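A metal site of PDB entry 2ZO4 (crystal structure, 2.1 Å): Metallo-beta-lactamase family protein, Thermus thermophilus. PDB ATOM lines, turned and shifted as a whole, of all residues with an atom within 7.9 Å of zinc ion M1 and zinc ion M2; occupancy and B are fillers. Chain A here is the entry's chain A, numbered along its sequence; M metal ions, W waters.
The side-chain carboxylate (OD2) of Asp 37 is in hydrogen-bond range of a ring nitrogen (ND1) of His 75 (2.6 Å). The backbone NH (N) of Asp 190 sits at hydrogen-bond distance from a ring nitrogen (NE2) of His 175. The backbone carbonyl oxygen (O) of Asn 199 sits at hydrogen-bond distance from a ring nitrogen (ND1) of His 171. ND1 of His 233 is in hydrogen-bond range of O of Thr 21, 2.7 Å away. The side-chain hydroxyl of Thr 69 sits at hydrogen-bond distance from a ring nitrogen (ND1) of His 70.
The nearest printed residue that does not touch zinc ion M2 is His 75 (4.1 Å).
Zinc ion M1 is bound by water W1 (2.0 Å), NE2 of His 75 (2.1 Å), OD2 of Asp 190 (2.1 Å), NE2 of His 233 (2.1 Å) and OD2 of Asp 74 (2.3 Å). Zinc ion M1 has five donor atoms within binding distance.
Zinc ion M2 is bound by water W1 (2.0 Å), NE2 of His 171 (2.1 Å), ND1 of His 72 (2.2 Å), NE2 of His 70 (2.2 Å) and OD2 of Asp 190 (2.6 Å). Zinc ion M2 has five donor atoms within binding distance.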
ATOM      1  N   ILE A  15     -19.892 -22.654   4.708  1.00  0.00           N
ATOM      2  CA  ILE A  15     -21.296 -22.366   5.018  1.00  0.00           C
ATOM      3  C   ILE A  15     -22.135 -22.297   3.721  1.00  0.00           C
ATOM      4  O   ILE A  15     -21.647 -21.806   2.699  1.00  0.00           O
ATOM      5  CB  ILE A  15     -21.474 -21.077   5.874  1.00  0.00           C
ATOM      6  CG1 ILE A  15     -20.824 -19.861   5.190  1.00  0.00           C
ATOM      7  CG2 ILE A  15     -20.928 -21.290   7.273  1.00  0.00           C
ATOM      8  CD1 ILE A  15     -21.217 -18.516   5.806  1.00  0.00           C
ATOM      9  N   LEU A  19     -21.731 -15.908   1.476  1.00  0.00           N
ATOM     10  CA  LEU A  19     -20.442 -15.603   2.111  1.00  0.00           C
ATOM     11  C   LEU A  19     -19.451 -16.778   2.018  1.00  0.00           C
ATOM     12  O   LEU A  19     -18.232 -16.577   2.070  1.00  0.00           O
ATOM     13  CB  LEU A  19     -20.636 -15.174   3.572  1.00  0.00           C
ATOM     14  N   THR A  21     -17.814 -18.925   3.550  1.00  0.00           N
ATOM     15  CA  THR A  21     -16.920 -19.333   4.633  1.00  0.00           C
ATOM     16  C   THR A  21     -17.083 -18.420   5.850  1.00  0.00           C
ATOM     17  O   THR A  21     -17.076 -17.189   5.730  1.00  0.00           O
ATOM     18  CB  THR A  21     -15.435 -19.320   4.177  1.00  0.00           C
ATOM     19  OG1 THR A  21     -15.299 -20.042   2.943  1.00  0.00           O
ATOM     20  CG2 THR A  21     -14.530 -19.959   5.226  1.00  0.00           C
ATOM     21  N   VAL A  22     -17.232 -19.040   7.017  1.00  0.00           N
ATOM     22  CA  VAL A  22     -17.244 -18.321   8.283  1.00  0.00           C
ATOM     23  C   VAL A  22     -15.927 -18.554   9.017  1.00  0.00           C
ATOM     24  O   VAL A  22     -15.358 -19.646   8.955  1.00  0.00           O
ATOM     25  CB  VAL A  22     -18.481 -18.698   9.159  1.00  0.00           C
ATOM     26  CG1 VAL A  22     -18.386 -20.147   9.684  1.00  0.00           C
ATOM     27  CG2 VAL A  22     -18.674 -17.697  10.303  1.00  0.00           C
ATOM     28  N   ASN A  23     -15.449 -17.508   9.688  1.00  0.00           N
ATOM     29  CA  ASN A  23     -14.248 -17.586  10.514  1.00  0.00           C
ATOM     30  C   ASN A  23     -14.576 -17.753  11.993  1.00  0.00           C
ATOM     31  O   ASN A  23     -15.171 -16.845  12.617  1.00  0.00           O
ATOM     32  CB  ASN A  23     -13.376 -16.334  10.333  1.00  0.00           C
ATOM     33  CG  ASN A  23     -12.848 -16.193   8.925  1.00  0.00           C
ATOM     34  OD1 ASN A  23     -12.551 -17.178   8.259  1.00  0.00           O
ATOM     35  ND2 ASN A  23     -12.743 -14.951   8.459  1.00  0.00           N
ATOM     36  N   ASP A  37     -17.728 -18.175  18.169  1.00  0.00           N
ATOM     37  CA  ASP A  37     -18.636 -18.620  17.093  1.00  0.00           C
ATOM     38  C   ASP A  37     -18.498 -20.125  16.770  1.00  0.00           C
ATOM     39  O   ASP A  37     -17.511 -20.752  17.138  1.00  0.00           O
ATOM     40  CB  ASP A  37     -18.530 -17.713  15.861  1.00  0.00           C
ATOM     41  CG  ASP A  37     -18.977 -16.277  16.159  1.00  0.00           C
ATOM     42  OD1 ASP A  37     -19.736 -16.092  17.131  1.00  0.00           O
ATOM     43  OD2 ASP A  37     -18.568 -15.351  15.422  1.00  0.00           O
ATOM     44  N   THR A  69     -20.629 -13.928  18.846  1.00  0.00           N
ATOM     45  CA  THR A  69     -20.681 -12.542  18.404  1.00  0.00           C
ATOM     46  C   THR A  69     -22.115 -12.103  18.141  1.00  0.00           C
ATOM     47  O   THR A  69     -22.506 -10.994  18.506  1.00  0.00           O
ATOM     48  CB  THR A  69     -19.809 -12.297  17.148  1.00  0.00           C
ATOM     49  OG1 THR A  69     -20.257 -13.119  16.073  1.00  0.00           O
ATOM     50  CG2 THR A  69     -18.331 -12.589  17.451  1.00  0.00           C
ATOM     51  N   HIS A  70     -22.905 -12.994  17.530  1.00  0.00           N
ATOM     52  CA  HIS A  70     -24.322 -12.733  17.242  1.00  0.00           C
ATOM     53  C   HIS A  70     -25.105 -14.005  16.884  1.00  0.00           C
ATOM     54  O   HIS A  70     -24.553 -15.107  16.827  1.00  0.00           O
ATOM     55  CB  HIS A  70     -24.471 -11.653  16.161  1.00  0.00           C
ATOM     56  CG  HIS A  70     -23.830 -11.973  14.844  1.00  0.00           C
ATOM     57  ND1 HIS A  70     -22.497 -12.301  14.720  1.00  0.00           N
ATOM     58  CD2 HIS A  70     -24.331 -11.985  13.593  1.00  0.00           C
ATOM     59  CE1 HIS A  70     -22.203 -12.511  13.454  1.00  0.00           C
ATOM     60  NE2 HIS A  70     -23.308 -12.327  12.746  1.00  0.00           N
ATOM     61  N   HIS A  71     -26.406 -13.817  16.621  1.00  0.00           N
ATOM     62  CA  HIS A  71     -27.376 -14.901  16.461  1.00  0.00           C
ATOM     63  C   HIS A  71     -27.490 -15.479  15.048  1.00  0.00           C
ATOM     64  O   HIS A  71     -28.254 -16.427  14.840  1.00  0.00           O
ATOM     65  CB  HIS A  71     -28.763 -14.413  16.866  1.00  0.00           C
ATOM     66  CG  HIS A  71     -29.402 -13.510  15.859  1.00  0.00           C
ATOM     67  ND1 HIS A  71     -29.109 -12.167  15.773  1.00  0.00           N
ATOM     68  CD2 HIS A  71     -30.292 -13.761  14.871  1.00  0.00           C
ATOM     69  CE1 HIS A  71     -29.799 -11.620  14.790  1.00  0.00           C
ATOM     70  NE2 HIS A  71     -30.523 -12.566  14.231  1.00  0.00           N
ATOM     71  N   HIS A  72     -26.802 -14.887  14.078  1.00  0.00           N
ATOM     72  CA  HIS A  72     -26.921 -15.362  12.695  1.00  0.00           C
ATOM     73  C   HIS A  72     -26.466 -16.828  12.618  1.00  0.00           C
ATOM     74  O   HIS A  72     -25.552 -17.228  13.340  1.00  0.00           O
ATOM     75  CB  HIS A  72     -26.163 -14.462  11.707  1.00  0.00           C
ATOM     76  CG  HIS A  72     -26.739 -13.094  11.569  1.00  0.00           C
ATOM     77  ND1 HIS A  72     -26.062 -12.057  10.961  1.00  0.00           N
ATOM     78  CD2 HIS A  72     -27.929 -12.569  11.975  1.00  0.00           C
ATOM     79  CE1 HIS A  72     -26.816 -10.966  10.979  1.00  0.00           C
ATOM     80  NE2 HIS A  72     -27.947 -11.259  11.597  1.00  0.00           N
ATOM     81  N   PRO A  73     -27.110 -17.626  11.736  1.00  0.00           N
ATOM     82  CA  PRO A  73     -26.931 -19.082  11.735  1.00  0.00           C
ATOM     83  C   PRO A  73     -25.482 -19.536  11.575  1.00  0.00           C
ATOM     84  O   PRO A  73     -25.078 -20.533  12.185  1.00  0.00           O
ATOM     85  CB  PRO A  73     -27.789 -19.547  10.552  1.00  0.00           C
ATOM     86  CG  PRO A  73     -27.997 -18.322   9.711  1.00  0.00           C
ATOM     87  CD  PRO A  73     -28.030 -17.186  10.672  1.00  0.00           C
ATOM     88  N   ASP A  74     -24.702 -18.828  10.768  1.00  0.00           N
ATOM     89  CA  ASP A  74     -23.289 -19.149  10.532  1.00  0.00           C
ATOM     90  C   ASP A  74     -22.364 -18.952  11.743  1.00  0.00           C
ATOM     91  O   ASP A  74     -21.206 -19.378  11.721  1.00  0.00           O
ATOM     92  CB  ASP A  74     -22.750 -18.379   9.308  1.00  0.00           C
ATOM     93  CG  ASP A  74     -22.998 -16.871   9.382  1.00  0.00           C
ATOM     94  OD1 ASP A  74     -24.077 -16.442   9.861  1.00  0.00           O
ATOM     95  OD2 ASP A  74     -22.110 -16.111   8.952  1.00  0.00           O
ATOM     96  N   HIS A  75     -22.871 -18.324  12.795  1.00  0.00           N
ATOM     97  CA  HIS A  75     -22.094 -18.078  14.021  1.00  0.00           C
ATOM     98  C   HIS A  75     -22.716 -18.805  15.228  1.00  0.00           C
ATOM     99  O   HIS A  75     -22.010 -19.222  16.136  1.00  0.00           O
ATOM    100  CB  HIS A  75     -22.016 -16.571  14.298  1.00  0.00           C
ATOM    101  CG  HIS A  75     -21.383 -15.787  13.194  1.00  0.00           C
ATOM    102  ND1 HIS A  75     -20.070 -15.347  13.242  1.00  0.00           N
ATOM    103  CD2 HIS A  75     -21.870 -15.357  12.010  1.00  0.00           C
ATOM    104  CE1 HIS A  75     -19.790 -14.692  12.131  1.00  0.00           C
ATOM    105  NE2 HIS A  75     -20.864 -14.683  11.371  1.00  0.00           N
ATOM    106  N   HIS A 171     -25.337  -4.704  12.549  1.00  0.00           N
ATOM    107  CA  HIS A 171     -25.381  -5.963  11.819  1.00  0.00           C
ATOM    108  C   HIS A 171     -26.339  -6.943  12.502  1.00  0.00           C
ATOM    109  O   HIS A 171     -27.075  -7.673  11.839  1.00  0.00           O
ATOM    110  CB  HIS A 171     -23.984  -6.561  11.709  1.00  0.00           C
ATOM    111  CG  HIS A 171     -23.958  -7.869  10.986  1.00  0.00           C
ATOM    112  ND1 HIS A 171     -24.074  -7.971   9.619  1.00  0.00           N
ATOM    113  CD2 HIS A 171     -23.836  -9.141  11.450  1.00  0.00           C
ATOM    114  CE1 HIS A 171     -24.024  -9.237   9.262  1.00  0.00           C
ATOM    115  NE2 HIS A 171     -23.870  -9.968  10.354  1.00  0.00           N
ATOM    116  N   ALA A 172     -26.311  -6.958  13.830  1.00  0.00           N
ATOM    117  CA  ALA A 172     -27.313  -7.643  14.646  1.00  0.00           C
ATOM    118  C   ALA A 172     -27.505  -6.833  15.910  1.00  0.00           C
ATOM    119  O   ALA A 172     -26.615  -6.097  16.316  1.00  0.00           O
ATOM    120  CB  ALA A 172     -26.875  -9.077  14.976  1.00  0.00           C
ATOM    121  N   HIS A 175     -25.098  -7.714  18.696  1.00  0.00           N
ATOM    122  CA  HIS A 175     -23.800  -8.089  18.165  1.00  0.00           C
ATOM    123  C   HIS A 175     -22.719  -7.623  19.139  1.00  0.00           C
ATOM    124  O   HIS A 175     -22.727  -6.481  19.606  1.00  0.00           O
ATOM    125  CB  HIS A 175     -23.565  -7.531  16.773  1.00  0.00           C
ATOM    126  CG  HIS A 175     -22.296  -8.007  16.149  1.00  0.00           C
ATOM    127  ND1 HIS A 175     -21.069  -7.446  16.424  1.00  0.00           N
ATOM    128  CD2 HIS A 175     -22.050  -9.022  15.279  1.00  0.00           C
ATOM    129  CE1 HIS A 175     -20.133  -8.086  15.746  1.00  0.00           C
ATOM    130  NE2 HIS A 175     -20.704  -9.037  15.049  1.00  0.00           N
ATOM    131  N   GLY A 189     -16.176 -10.104  14.821  1.00  0.00           N
ATOM    132  CA  GLY A 189     -17.408 -10.733  14.333  1.00  0.00           C
ATOM    133  C   GLY A 189     -17.764 -10.160  12.966  1.00  0.00           C
ATOM    134  O   GLY A 189     -16.892 -10.006  12.124  1.00  0.00           O
ATOM    135  N   ASP A 190     -19.034  -9.834  12.763  1.00  0.00           N
ATOM    136  CA  ASP A 190     -19.451  -9.192  11.525  1.00  0.00           C
ATOM    137  C   ASP A 190     -19.722  -7.695  11.658  1.00  0.00           C
ATOM    138  O   ASP A 190     -20.453  -7.120  10.861  1.00  0.00           O
ATOM    139  CB  ASP A 190     -20.687  -9.890  10.933  1.00  0.00           C
ATOM    140  CG  ASP A 190     -20.409 -11.327  10.498  1.00  0.00           C
ATOM    141  OD1 ASP A 190     -19.258 -11.811  10.637  1.00  0.00           O
ATOM    142  OD2 ASP A 190     -21.359 -11.969  10.019  1.00  0.00           O
ATOM    143  N   ALA A 191     -19.146  -7.048  12.676  1.00  0.00           N
ATOM    144  CA  ALA A 191     -19.281  -5.594  12.841  1.00  0.00           C
ATOM    145  C   ALA A 191     -18.421  -4.854  11.817  1.00  0.00           C
ATOM    146  O   ALA A 191     -18.648  -3.676  11.524  1.00  0.00           O
ATOM    147  CB  ALA A 191     -18.896  -5.186  14.266  1.00  0.00           C
ATOM    148  N   LEU A 193     -15.898  -5.946   8.160  1.00  0.00           N
ATOM    149  CA  LEU A 193     -15.339  -6.906   7.189  1.00  0.00           C
ATOM    150  C   LEU A 193     -14.446  -6.157   6.207  1.00  0.00           C
ATOM    151  O   LEU A 193     -14.675  -4.975   5.951  1.00  0.00           O
ATOM    152  CB  LEU A 193     -16.452  -7.633   6.433  1.00  0.00           C
ATOM    153  CG  LEU A 193     -17.446  -8.547   7.171  1.00  0.00           C
ATOM    154  CD1 LEU A 193     -18.542  -9.009   6.231  1.00  0.00           C
ATOM    155  CD2 LEU A 193     -16.749  -9.734   7.819  1.00  0.00           C
ATOM    156  N   PRO A 198     -20.642  -5.796   5.898  1.00  0.00           N
ATOM    157  CA  PRO A 198     -21.563  -6.732   6.522  1.00  0.00           C
ATOM    158  C   PRO A 198     -22.993  -6.210   6.391  1.00  0.00           C
ATOM    159  O   PRO A 198     -23.211  -4.992   6.380  1.00  0.00           O
ATOM    160  CB  PRO A 198     -21.126  -6.751   7.994  1.00  0.00           C
ATOM    161  CG  PRO A 198     -20.277  -5.542   8.177  1.00  0.00           C
ATOM    162  CD  PRO A 198     -19.637  -5.275   6.859  1.00  0.00           C
ATOM    163  N   ASN A 199     -23.946  -7.123   6.270  1.00  0.00           N
ATOM    164  CA  ASN A 199     -25.358  -6.776   6.194  1.00  0.00           C
ATOM    165  C   ASN A 199     -25.768  -5.831   7.323  1.00  0.00           C
ATOM    166  O   ASN A 199     -25.308  -5.967   8.466  1.00  0.00           O
ATOM    167  CB  ASN A 199     -26.217  -8.043   6.240  1.00  0.00           C
ATOM    168  CG  ASN A 199     -27.550  -7.888   5.532  1.00  0.00           C
ATOM    169  OD1 ASN A 199     -27.608  -7.710   4.309  1.00  0.00           O
ATOM    170  ND2 ASN A 199     -28.647  -7.964   6.291  1.00  0.00           N
ATOM    171  N   ALA A 231     -12.123 -10.891  11.635  1.00  0.00           N
ATOM    172  CA  ALA A 231     -13.569 -10.802  11.525  1.00  0.00           C
ATOM    173  C   ALA A 231     -14.221 -12.156  11.219  1.00  0.00           C
ATOM    174  O   ALA A 231     -13.526 -13.167  11.100  1.00  0.00           O
ATOM    175  CB  ALA A 231     -13.946  -9.771  10.477  1.00  0.00           C
ATOM    176  N   GLY A 232     -15.541 -12.155  11.097  1.00  0.00           N
ATOM    177  CA  GLY A 232     -16.314 -13.373  10.871  1.00  0.00           C
ATOM    178  C   GLY A 232     -16.211 -13.919   9.468  1.00  0.00           C
ATOM    179  O   GLY A 232     -16.482 -15.099   9.231  1.00  0.00           O
ATOM    180  N   HIS A 233     -15.816 -13.060   8.527  1.00  0.00           N
ATOM    181  CA  HIS A 233     -15.632 -13.476   7.134  1.00  0.00           C
ATOM    182  C   HIS A 233     -14.439 -12.757   6.512  1.00  0.00           C
ATOM    183  O   HIS A 233     -14.027 -11.693   6.986  1.00  0.00           O
ATOM    184  CB  HIS A 233     -16.897 -13.196   6.315  1.00  0.00           C
ATOM    185  CG  HIS A 233     -18.136 -13.783   6.901  1.00  0.00           C
ATOM    186  ND1 HIS A 233     -18.490 -15.101   6.743  1.00  0.00           N
ATOM    187  CD2 HIS A 233     -19.104 -13.220   7.668  1.00  0.00           C
ATOM    188  CE1 HIS A 233     -19.625 -15.340   7.379  1.00  0.00           C
ATOM    189  NE2 HIS A 233     -20.017 -14.215   7.949  1.00  0.00           N
ATOM    190  N   PHE A 287     -31.519 -10.701   1.971  1.00  0.00           N
ATOM    191  CA  PHE A 287     -30.580  -9.790   2.627  1.00  0.00           C
ATOM    192  C   PHE A 287     -30.549  -8.426   1.950  1.00  0.00           C
ATOM    193  O   PHE A 287     -30.471  -7.397   2.609  1.00  0.00           O
ATOM    194  CB  PHE A 287     -29.174 -10.394   2.676  1.00  0.00           C
ATOM    195  CG  PHE A 287     -29.117 -11.724   3.385  1.00  0.00           C
ATOM    196  CD1 PHE A 287     -28.785 -12.883   2.681  1.00  0.00           C
ATOM    197  CD2 PHE A 287     -29.406 -11.824   4.744  1.00  0.00           C
ATOM    198  CE1 PHE A 287     -28.739 -14.115   3.324  1.00  0.00           C
ATOM    199  CE2 PHE A 287     -29.367 -13.061   5.390  1.00  0.00           C
ATOM    200  CZ  PHE A 287     -29.027 -14.215   4.683  1.00  0.00           C
HETATM  201 ZN    ZN M   1     -21.411 -13.972   9.514  1.00  0.00          ZN
HETATM  202 ZN    ZN M   2     -23.863 -12.035  10.597  1.00  0.00          ZN
HETATM  203  O   HOH W   1     -23.357 -13.619   9.470  1.00  0.00           O
